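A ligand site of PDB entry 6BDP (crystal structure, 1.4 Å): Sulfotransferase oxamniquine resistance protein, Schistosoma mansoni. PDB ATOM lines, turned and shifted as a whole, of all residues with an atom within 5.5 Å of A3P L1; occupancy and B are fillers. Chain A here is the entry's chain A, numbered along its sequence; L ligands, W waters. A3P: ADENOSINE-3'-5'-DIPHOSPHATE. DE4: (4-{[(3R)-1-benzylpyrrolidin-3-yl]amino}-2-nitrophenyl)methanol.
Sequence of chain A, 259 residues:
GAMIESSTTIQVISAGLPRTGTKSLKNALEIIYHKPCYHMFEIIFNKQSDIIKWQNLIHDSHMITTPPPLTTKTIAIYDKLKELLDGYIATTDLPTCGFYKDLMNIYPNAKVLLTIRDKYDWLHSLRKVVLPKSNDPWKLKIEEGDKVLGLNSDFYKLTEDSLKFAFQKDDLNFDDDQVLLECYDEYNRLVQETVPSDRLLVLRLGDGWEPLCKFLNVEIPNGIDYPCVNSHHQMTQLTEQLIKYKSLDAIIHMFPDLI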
ATOM      1  N   LEU A  17      23.648   3.074 -15.213  1.00  0.00           N
ATOM      2  CA  LEU A  17      22.814   3.598 -16.287  1.00  0.00           C
ATOM      3  C   LEU A  17      22.374   5.043 -15.988  1.00  0.00           C
ATOM      4  O   LEU A  17      22.441   5.504 -14.847  1.00  0.00           O
ATOM      5  CB  LEU A  17      21.586   2.710 -16.435  1.00  0.00           C
ATOM      6  CG  LEU A  17      21.868   1.325 -17.005  1.00  0.00           C
ATOM      7  CD1 LEU A  17      20.711   0.302 -16.811  1.00  0.00           C
ATOM      8  CD2 LEU A  17      22.268   1.436 -18.470  1.00  0.00           C
ATOM      9  N   PRO A  18      21.946   5.785 -16.995  1.00  0.00           N
ATOM     10  CA  PRO A  18      21.436   7.130 -16.731  1.00  0.00           C
ATOM     11  C   PRO A  18      20.281   7.095 -15.740  1.00  0.00           C
ATOM     12  O   PRO A  18      19.517   6.133 -15.671  1.00  0.00           O
ATOM     13  CB  PRO A  18      20.971   7.611 -18.108  1.00  0.00           C
ATOM     14  CG  PRO A  18      20.853   6.387 -18.938  1.00  0.00           C
ATOM     15  CD  PRO A  18      21.908   5.465 -18.436  1.00  0.00           C
ATOM     16  N   ARG A  19      20.175   8.170 -14.954  1.00  0.00           N
ATOM     17  CA  ARG A  19      19.140   8.348 -13.932  1.00  0.00           C
ATOM     18  C   ARG A  19      19.363   7.460 -12.710  1.00  0.00           C
ATOM     19  O   ARG A  19      18.403   7.102 -12.016  1.00  0.00           O
ATOM     20  CB  ARG A  19      17.716   8.205 -14.468  1.00  0.00           C
ATOM     21  CG  ARG A  19      17.435   8.974 -15.753  1.00  0.00           C
ATOM     22  CD  ARG A  19      17.822  10.454 -15.693  1.00  0.00           C
ATOM     23  NE  ARG A  19      17.119  11.192 -14.658  1.00  0.00           N
ATOM     24  CZ  ARG A  19      17.358  12.462 -14.311  1.00  0.00           C
ATOM     25  NH1 ARG A  19      18.326  13.155 -14.888  1.00  0.00           N
ATOM     26  NH2 ARG A  19      16.614  13.041 -13.371  1.00  0.00           N
ATOM     27  N   THR A  20      20.620   7.112 -12.434  1.00  0.00           N
ATOM     28  CA  THR A  20      21.012   6.398 -11.213  1.00  0.00           C
ATOM     29  C   THR A  20      21.993   7.183 -10.342  1.00  0.00           C
ATOM     30  O   THR A  20      22.680   6.576  -9.524  1.00  0.00           O
ATOM     31  CB  THR A  20      21.598   5.019 -11.522  1.00  0.00           C
ATOM     32  OG1 THR A  20      22.815   5.166 -12.269  1.00  0.00           O
ATOM     33  CG2 THR A  20      20.596   4.170 -12.312  1.00  0.00           C
ATOM     34  N   GLY A  21      22.069   8.497 -10.482  1.00  0.00           N
ATOM     35  CA  GLY A  21      23.042   9.290  -9.739  1.00  0.00           C
ATOM     36  C   GLY A  21      24.334   9.554 -10.492  1.00  0.00           C
ATOM     37  O   GLY A  21      25.349   9.857  -9.849  1.00  0.00           O
ATOM     38  N   THR A  22      24.334   9.456 -11.830  1.00  0.00           N
ATOM     39  CA  THR A  22      25.581   9.609 -12.599  1.00  0.00           C
ATOM     40  C   THR A  22      26.129  11.030 -12.529  1.00  0.00           C
ATOM     41  O   THR A  22      27.348  11.219 -12.481  1.00  0.00           O
ATOM     42  CB  THR A  22      25.414   9.151 -14.065  1.00  0.00           C
ATOM     43  OG1 THR A  22      24.511  10.018 -14.760  1.00  0.00           O
ATOM     44  CG2 THR A  22      24.920   7.719 -14.152  1.00  0.00           C
ATOM     45  N   LYS A  23      25.272  12.051 -12.569  1.00  0.00           N
ATOM     46  CA  LYS A  23      25.783  13.419 -12.548  1.00  0.00           C
ATOM     47  C   LYS A  23      26.365  13.777 -11.179  1.00  0.00           C
ATOM     48  O   LYS A  23      27.406  14.433 -11.085  1.00  0.00           O
ATOM     49  CB  LYS A  23      24.706  14.394 -13.019  1.00  0.00           C
ATOM     50  CG  LYS A  23      25.137  15.877 -13.082  1.00  0.00           C
ATOM     51  CD  LYS A  23      26.375  16.079 -13.921  1.00  0.00           C
ATOM     52  CE  LYS A  23      26.614  17.489 -14.431  1.00  0.00           C
ATOM     53  NZ  LYS A  23      27.294  18.430 -13.538  1.00  0.00           N
ATOM     54  N   SER A  24      25.700  13.351 -10.118  1.00  0.00           N
ATOM     55  CA  SER A  24      26.253  13.566  -8.786  1.00  0.00           C
ATOM     56  C   SER A  24      27.591  12.841  -8.647  1.00  0.00           C
ATOM     57  O   SER A  24      28.537  13.377  -8.060  1.00  0.00           O
ATOM     58  CB  SER A  24      25.296  13.061  -7.709  1.00  0.00           C
ATOM     59  OG  SER A  24      24.136  13.860  -7.637  1.00  0.00           O
ATOM     60  N   HIS A  39      30.525  12.288 -19.034  1.00  0.00           N
ATOM     61  CA  HIS A  39      29.090  12.237 -18.741  1.00  0.00           C
ATOM     62  C   HIS A  39      28.385  12.718 -19.991  1.00  0.00           C
ATOM     63  O   HIS A  39      28.992  13.408 -20.815  1.00  0.00           O
ATOM     64  CB  HIS A  39      28.759  13.155 -17.559  1.00  0.00           C
ATOM     65  CG  HIS A  39      27.370  12.976 -17.026  1.00  0.00           C
ATOM     66  ND1 HIS A  39      26.295  13.714 -17.483  1.00  0.00           N
ATOM     67  CD2 HIS A  39      26.889  12.173 -16.040  1.00  0.00           C
ATOM     68  CE1 HIS A  39      25.209  13.329 -16.841  1.00  0.00           C
ATOM     69  NE2 HIS A  39      25.536  12.420 -15.959  1.00  0.00           N
ATOM     70  N   ARG A 117      19.484   1.766  -8.286  1.00  0.00           N
ATOM     71  CA  ARG A 117      18.358   2.278  -7.513  1.00  0.00           C
ATOM     72  C   ARG A 117      17.129   1.409  -7.796  1.00  0.00           C
ATOM     73  O   ARG A 117      17.135   0.541  -8.671  1.00  0.00           O
ATOM     74  CB  ARG A 117      18.066   3.756  -7.818  1.00  0.00           C
ATOM     75  CG  ARG A 117      17.432   3.960  -9.165  1.00  0.00           C
ATOM     76  CD  ARG A 117      17.288   5.399  -9.588  1.00  0.00           C
ATOM     77  NE  ARG A 117      16.374   6.166  -8.751  1.00  0.00           N
ATOM     78  CZ  ARG A 117      16.026   7.426  -9.005  1.00  0.00           C
ATOM     79  NH1 ARG A 117      16.428   8.034 -10.113  1.00  0.00           N
ATOM     80  NH2 ARG A 117      15.201   8.055  -8.189  1.00  0.00           N
ATOM     81  N   ASP A 121      11.479   3.781  -9.603  1.00  0.00           N
ATOM     82  CA  ASP A 121      11.975   5.158  -9.512  1.00  0.00           C
ATOM     83  C   ASP A 121      12.834   5.488 -10.736  1.00  0.00           C
ATOM     84  O   ASP A 121      12.769   6.599 -11.270  1.00  0.00           O
ATOM     85  CB  ASP A 121      12.812   5.350  -8.254  1.00  0.00           C
ATOM     86  CG  ASP A 121      12.006   5.328  -6.955  1.00  0.00           C
ATOM     87  OD1 ASP A 121      10.757   5.418  -6.977  1.00  0.00           O
ATOM     88  OD2 ASP A 121      12.637   5.225  -5.880  1.00  0.00           O
ATOM     89  N   SER A 125      11.974   8.376 -13.545  1.00  0.00           N
ATOM     90  CA  SER A 125      12.960   9.413 -13.820  1.00  0.00           C
ATOM     91  C   SER A 125      13.340   9.425 -15.293  1.00  0.00           C
ATOM     92  O   SER A 125      13.402  10.487 -15.921  1.00  0.00           O
ATOM     93  CB  SER A 125      14.184   9.138 -12.945  1.00  0.00           C
ATOM     94  OG  SER A 125      15.173  10.143 -13.023  1.00  0.00           O
ATOM     95  N   VAL A 129      12.823  12.652 -18.218  1.00  0.00           N
ATOM     96  CA  VAL A 129      14.027  13.376 -18.614  1.00  0.00           C
ATOM     97  C   VAL A 129      14.586  12.904 -19.955  1.00  0.00           C
ATOM     98  O   VAL A 129      14.899  13.720 -20.821  1.00  0.00           O
ATOM     99  CB  VAL A 129      15.107  13.288 -17.527  1.00  0.00           C
ATOM    100  CG1 VAL A 129      16.392  14.020 -17.970  1.00  0.00           C
ATOM    101  CG2 VAL A 129      14.590  13.827 -16.259  1.00  0.00           C
ATOM    102  N   LEU A 205      21.761   5.133  -4.340  1.00  0.00           N
ATOM    103  CA  LEU A 205      21.530   6.551  -4.045  1.00  0.00           C
ATOM    104  C   LEU A 205      21.443   6.745  -2.542  1.00  0.00           C
ATOM    105  O   LEU A 205      20.755   6.001  -1.854  1.00  0.00           O
ATOM    106  CB  LEU A 205      20.241   7.053  -4.702  1.00  0.00           C
ATOM    107  CG  LEU A 205      20.257   7.188  -6.207  1.00  0.00           C
ATOM    108  CD1 LEU A 205      18.856   7.543  -6.716  1.00  0.00           C
ATOM    109  CD2 LEU A 205      21.318   8.210  -6.662  1.00  0.00           C
ATOM    110  N   GLY A 206      22.135   7.767  -2.046  1.00  0.00           N
ATOM    111  CA  GLY A 206      22.178   8.025  -0.621  1.00  0.00           C
ATOM    112  C   GLY A 206      23.433   7.538   0.059  1.00  0.00           C
ATOM    113  O   GLY A 206      23.672   7.912   1.221  1.00  0.00           O
ATOM    114  N   TYR A 226      28.304  15.377  -0.165  1.00  0.00           N
ATOM    115  CA  TYR A 226      28.213  14.600  -1.384  1.00  0.00           C
ATOM    116  C   TYR A 226      27.171  15.237  -2.307  1.00  0.00           C
ATOM    117  O   TYR A 226      26.100  15.640  -1.847  1.00  0.00           O
ATOM    118  CB  TYR A 226      27.811  13.155  -1.086  1.00  0.00           C
ATOM    119  CG  TYR A 226      27.892  12.276  -2.308  1.00  0.00           C
ATOM    120  CD1 TYR A 226      29.089  11.646  -2.674  1.00  0.00           C
ATOM    121  CD2 TYR A 226      26.796  12.101  -3.138  1.00  0.00           C
ATOM    122  CE1 TYR A 226      29.171  10.873  -3.798  1.00  0.00           C
ATOM    123  CE2 TYR A 226      26.884  11.330  -4.281  1.00  0.00           C
ATOM    124  CZ  TYR A 226      28.075  10.714  -4.605  1.00  0.00           C
ATOM    125  OH  TYR A 226      28.145   9.927  -5.745  1.00  0.00           O
ATOM    126  N   PRO A 227      27.469  15.372  -3.600  1.00  0.00           N
ATOM    127  CA  PRO A 227      26.520  16.049  -4.489  1.00  0.00           C
ATOM    128  C   PRO A 227      25.127  15.427  -4.613  1.00  0.00           C
ATOM    129  O   PRO A 227      24.965  14.225  -4.538  1.00  0.00           O
ATOM    130  CB  PRO A 227      27.216  15.989  -5.853  1.00  0.00           C
ATOM    131  CG  PRO A 227      28.671  15.847  -5.522  1.00  0.00           C
ATOM    132  CD  PRO A 227      28.712  15.010  -4.287  1.00  0.00           C
ATOM    133  N   CAS A 228      24.114  16.278  -4.784  1.00  0.00           N
ATOM    134  CA  CAS A 228      22.741  15.868  -5.033  1.00  0.00           C
ATOM    135  CB  CAS A 228      21.772  15.997  -3.870  1.00  0.00           C
ATOM    136  C   CAS A 228      22.276  16.795  -6.112  1.00  0.00           C
ATOM    137  O   CAS A 228      21.882  17.930  -5.817  1.00  0.00           O
ATOM    138  SG  CAS A 228      20.235  15.272  -4.366  1.00  0.00           S
ATOM    139 AS   CAS A 228      18.881  17.025  -4.666  1.00  0.00          AS
ATOM    140  CE1 CAS A 228      18.893  17.446  -6.611  1.00  0.00           C
ATOM    141  CE2 CAS A 228      17.068  16.249  -4.347  1.00  0.00           C
ATOM    142  N   VAL A 229      22.372  16.375  -7.367  1.00  0.00           N
ATOM    143  CA  VAL A 229      21.973  17.216  -8.479  1.00  0.00           C
ATOM    144  C   VAL A 229      21.289  16.386  -9.539  1.00  0.00           C
ATOM    145  O   VAL A 229      21.374  15.167  -9.517  1.00  0.00           O
ATOM    146  CB  VAL A 229      23.205  17.857  -9.171  1.00  0.00           C
ATOM    147  CG1 VAL A 229      23.919  18.849  -8.262  1.00  0.00           C
ATOM    148  CG2 VAL A 229      24.162  16.790  -9.654  1.00  0.00           C
ATOM    149  N   ASN A 230      20.568  17.062 -10.433  1.00  0.00           N
ATOM    150  CA  ASN A 230      19.993  16.427 -11.613  1.00  0.00           C
ATOM    151  C   ASN A 230      18.728  15.630 -11.288  1.00  0.00           C
ATOM    152  O   ASN A 230      18.464  14.600 -11.928  1.00  0.00           O
ATOM    153  CB  ASN A 230      21.018  15.538 -12.327  1.00  0.00           C
ATOM    154  CG  ASN A 230      20.676  15.292 -13.800  1.00  0.00           C
ATOM    155  OD1 ASN A 230      19.778  15.919 -14.374  1.00  0.00           O
ATOM    156  ND2 ASN A 230      21.380  14.354 -14.396  1.00  0.00           N
ATOM    157  N   SER A 231      17.940  16.091 -10.334  1.00  0.00           N
ATOM    158  CA  SER A 231      16.615  15.514 -10.115  1.00  0.00           C
ATOM    159  C   SER A 231      15.723  15.806 -11.319  1.00  0.00           C
ATOM    160  O   SER A 231      15.933  16.772 -12.051  1.00  0.00           O
ATOM    161  CB  SER A 231      15.975  16.116  -8.877  1.00  0.00           C
ATOM    162  OG  SER A 231      15.660  17.491  -9.065  1.00  0.00           O
ATOM    163  N   HIS A 232      14.748  14.934 -11.535  1.00  0.00           N
ATOM    164  CA  HIS A 232      13.844  15.189 -12.654  1.00  0.00           C
ATOM    165  C   HIS A 232      13.108  16.519 -12.460  1.00  0.00           C
ATOM    166  O   HIS A 232      12.842  17.210 -13.445  1.00  0.00           O
ATOM    167  CB  HIS A 232      12.894  14.002 -12.923  1.00  0.00           C
ATOM    168  CG  HIS A 232      11.819  13.810 -11.905  1.00  0.00           C
ATOM    169  ND1 HIS A 232      10.716  14.631 -11.813  1.00  0.00           N
ATOM    170  CD2 HIS A 232      11.663  12.862 -10.934  1.00  0.00           C
ATOM    171  CE1 HIS A 232       9.933  14.213 -10.830  1.00  0.00           C
ATOM    172  NE2 HIS A 232      10.488  13.140 -10.289  1.00  0.00           N
ATOM    173  N   HIS A 233      12.798  16.909 -11.221  1.00  0.00           N
ATOM    174  CA  HIS A 233      12.199  18.215 -11.000  1.00  0.00           C
ATOM    175  C   HIS A 233      13.100  19.328 -11.513  1.00  0.00           C
ATOM    176  O   HIS A 233      12.647  20.275 -12.154  1.00  0.00           O
ATOM    177  CB  HIS A 233      11.885  18.427  -9.521  1.00  0.00           C
ATOM    178  CG  HIS A 233      10.803  17.523  -8.995  1.00  0.00           C
ATOM    179  ND1 HIS A 233       9.522  17.534  -9.500  1.00  0.00           N
ATOM    180  CD2 HIS A 233      10.817  16.616  -7.998  1.00  0.00           C
ATOM    181  CE1 HIS A 233       8.790  16.648  -8.833  1.00  0.00           C
ATOM    182  NE2 HIS A 233       9.555  16.092  -7.911  1.00  0.00           N
HETATM  183  P1  A3P L   1      15.044  11.629  -9.740  1.00  0.00           P
HETATM  184  O1P A3P L   1      14.199  10.472  -9.247  1.00  0.00           O
HETATM  185  O2P A3P L   1      14.867  11.929 -11.210  1.00  0.00           O
HETATM  186  O3P A3P L   1      14.983  12.866  -8.878  1.00  0.00           O
HETATM  187  P2  A3P L   1      21.514  10.931 -13.223  1.00  0.00           P
HETATM  188  O4P A3P L   1      22.203   9.615 -13.471  1.00  0.00           O
HETATM  189  O5P A3P L   1      22.411  12.049 -12.758  1.00  0.00           O
HETATM  190  O6P A3P L   1      20.566  11.324 -14.327  1.00  0.00           O
HETATM  191  O5' A3P L   1      20.588  10.609 -11.945  1.00  0.00           O
HETATM  192  C5' A3P L   1      19.659  11.571 -11.456  1.00  0.00           C
HETATM  193  C4' A3P L   1      18.787  10.927 -10.391  1.00  0.00           C
HETATM  194  O4' A3P L   1      19.561  10.606  -9.237  1.00  0.00           O
HETATM  195  C3' A3P L   1      17.698  11.878  -9.931  1.00  0.00           C
HETATM  196  O3' A3P L   1      16.550  11.086  -9.590  1.00  0.00           O
HETATM  197  C2' A3P L   1      18.295  12.479  -8.674  1.00  0.00           C
HETATM  198  O2' A3P L   1      17.293  12.995  -7.789  1.00  0.00           O
HETATM  199  C1' A3P L   1      19.027  11.283  -8.094  1.00  0.00           C
HETATM  200  N9  A3P L   1      20.126  11.676  -7.194  1.00  0.00           N
HETATM  201  C8  A3P L   1      21.290  12.237  -7.570  1.00  0.00           C
HETATM  202  N7  A3P L   1      22.082  12.470  -6.499  1.00  0.00           N
HETATM  203  C5  A3P L   1      21.427  12.034  -5.405  1.00  0.00           C
HETATM  204  C6  A3P L   1      21.704  11.976  -3.959  1.00  0.00           C
HETATM  205  N6  A3P L   1      22.881  12.444  -3.468  1.00  0.00           N
HETATM  206  N1  A3P L   1      20.756  11.453  -3.155  1.00  0.00           N
HETATM  207  C2  A3P L   1      19.593  10.992  -3.652  1.00  0.00           C
HETATM  208  N3  A3P L   1      19.265  11.004  -4.961  1.00  0.00           N
HETATM  209  C4  A3P L   1      20.134  11.508  -5.865  1.00  0.00           C
HETATM  210  C1  DE4 L   2      20.617  12.988 -20.274  1.00  0.00           C
HETATM  211  C10 DE4 L   2      18.506  19.091 -21.559  1.00  0.00           C
HETATM  212  C11 DE4 L   2      19.712  19.612 -21.105  1.00  0.00           C
HETATM  213  C12 DE4 L   2      20.411  18.970 -20.087  1.00  0.00           C
HETATM  214  C13 DE4 L   2      17.635  14.600 -22.741  1.00  0.00           C
HETATM  215  C14 DE4 L   2      18.103  16.025 -22.979  1.00  0.00           C
HETATM  216  C15 DE4 L   2      19.908  17.807 -19.533  1.00  0.00           C
HETATM  217  C16 DE4 L   2      15.760  15.938 -23.178  1.00  0.00           C
HETATM  218  C17 DE4 L   2      16.321  14.555 -23.485  1.00  0.00           C
HETATM  219  C18 DE4 L   2      18.702  17.286 -19.986  1.00  0.00           C
HETATM  220  C2  DE4 L   2      21.043  11.703 -20.556  1.00  0.00           C
HETATM  221  C3  DE4 L   2      20.658  11.078 -21.741  1.00  0.00           C
HETATM  222  C4  DE4 L   2      19.823  11.743 -22.629  1.00  0.00           C
HETATM  223  C5  DE4 L   2      19.383  13.021 -22.341  1.00  0.00           C
HETATM  224  C6  DE4 L   2      19.771  13.647 -21.166  1.00  0.00           C
HETATM  225  C7  DE4 L   2      21.958  10.995 -19.575  1.00  0.00           C
HETATM  226  C8  DE4 L   2      16.690  17.366 -21.517  1.00  0.00           C
HETATM  227  C9  DE4 L   2      18.003  17.929 -21.004  1.00  0.00           C
HETATM  228  N12 DE4 L   2      18.577  13.636 -23.237  1.00  0.00           N
HETATM  229  N15 DE4 L   2      16.876  16.838 -22.884  1.00  0.00           N
HETATM  230  N8  DE4 L   2      21.019   9.926 -22.059  1.00  0.00           N
HETATM  231  O10 DE4 L   2      21.322   9.662 -23.231  1.00  0.00           O
HETATM  232  O11 DE4 L   2      21.091   8.879 -21.135  1.00  0.00           O
HETATM  233  O9  DE4 L   2      22.582  11.908 -18.672  1.00  0.00           O
HETATM  234  O   HOH W   1      12.041   8.940  -9.896  1.00  0.00           O
HETATM  235  O   HOH W   2      20.502  11.248  -0.500  1.00  0.00           O
HETATM  236  O   HOH W   3      16.432  10.319  -4.826  1.00  0.00           O
HETATM  237  O   HOH W   4      20.817  12.513 -16.713  1.00  0.00           O
HETATM  238  O   HOH W   5      22.874  12.820 -10.267  1.00  0.00           O
HETATM  239  O   HOH W   6      14.042  11.309  -6.422  1.00  0.00           O
HETATM  240  O   HOH W   7      13.001  14.731  -8.503  1.00  0.00           O
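An oxygen (O2P) of A3P L1 lies within hydrogen-bond range of the side-chain hydroxyl of Ser 125, at 2.6 Å. An oxygen (O4P) of A3P L1 sits at hydrogen-bond distance from the backbone NH (N) of Thr 22 (2.7 Å). OG1 of Thr 22 lies within hydrogen-bond range of O4P of A3P L1. A nitrogen (N7) of A3P L1 lies within hydrogen-bond range of the side-chain hydroxyl (OG) of Ser 24 (2.7 Å). An oxygen (O1P) of A3P L1 is in salt-bridge range of the guanidinium group of Arg 117 (2.8 Å). The backbone NH (N) of Lys 23 lies within hydrogen-bond range of an oxygen (O5P) of A3P L1 (2.9 Å). N of Arg 19 is in hydrogen-bond range of O4P of A3P L1 (2.9 Å). The guanidinium group (NH1) of Arg 19 lies within salt-bridge range of an oxygen (O6P) of A3P L1 (2.9 Å). The backbone carbonyl oxygen (O) of Pro 227 sits at hydrogen-bond distance from a nitrogen (N6) of A3P L1, at 2.9 Å. An oxygen (O5') of A3P L1 is in hydrogen-bond range of the backbone NH (N) of Gly 21. O5P of A3P L1 is in hydrogen-bond range of ND2 of Asn 230 (3.0 Å). N of His 232 lies within hydrogen-bond range of O2P of A3P L1. N of Thr 20 is in hydrogen-bond range of O4P of A3P L1, 3.1 Å away.
The side-chain hydroxyl (OG) of Ser 125 sits at hydrogen-bond distance from the guanidinium group (NE) of Arg 19, 2.7 Å away. OG1 of Thr 22 is in hydrogen-bond range of NE2 of His 39. The backbone carbonyl oxygen (O) of Pro 227 is in hydrogen-bond range of the side-chain hydroxyl (OG) of Ser 24, at 3.2 Å. The side-chain hydroxyl (OG) of Ser 24 is in hydrogen-bond range of the backbone NH (N) of Val 229 (3.1 Å). NH1 of Arg 117 sits at hydrogen-bond distance from O of Arg 19. N of Lys 23 sits at hydrogen-bond distance from NE2 of His 39. The backbone carbonyl oxygen of Asn 230 sits at hydrogen-bond distance from the guanidinium group of Arg 19. OG1 of Thr 20 sits at hydrogen-bond distance from O of Leu 17, 2.6 Å away.
Water W5 lies within hydrogen-bond range of O5P of A3P L1 (2.6 Å), N of Ser 24 (2.9 Å), O of Val 229 (2.9 Å) and N of Lys 23 (3.4 Å). Water W4 lies within hydrogen-bond range of O6P of A3P L1 (2.7 Å), O9 of DE4 L2 (2.7 Å), ND2 of Asn 230 (3.0 Å) and NH1 of Arg 19 (3.2 Å). Water W1 lies within hydrogen-bond range of an oxygen (O1P) of A3P L1 (2.7 Å) and the backbone carbonyl oxygen of Asp 121 (2.8 Å). Water W7 lies within hydrogen-bond range of an oxygen (O3P) of A3P L1 (2.7 Å), a ring nitrogen (NE2) of His 232 (3.5 Å) and the backbone NH (N) of His 233 (3.5 Å).
C of Pro 18 touches O4P of A3P L1, 3.9 Å away. Leu 205 touches A3P L1. CD2 of Tyr 226 touches N6 of A3P L1, at 3.9 Å. CAS 228 touches A3P L1. Val 229 touches A3P L1 (O to C8, 3.5 Å). Ser 231 touches A3P L1. Hydrophobic or aromatic side chains that line A3P L1: Leu 205, Tyr 226 and His 232. Within 4 Å of A3P L1: Pro 18, Arg 19, Thr 20, Gly 21, Thr 22, Lys 23, Ser 24, Arg 117, Ser 125, Leu 205, Tyr 226, Pro 227, CAS 228, Val 229, Asn 230, Ser 231 and His 232. Along chain A the residues within 4 Å of A3P L1 span positions 18 to 232.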
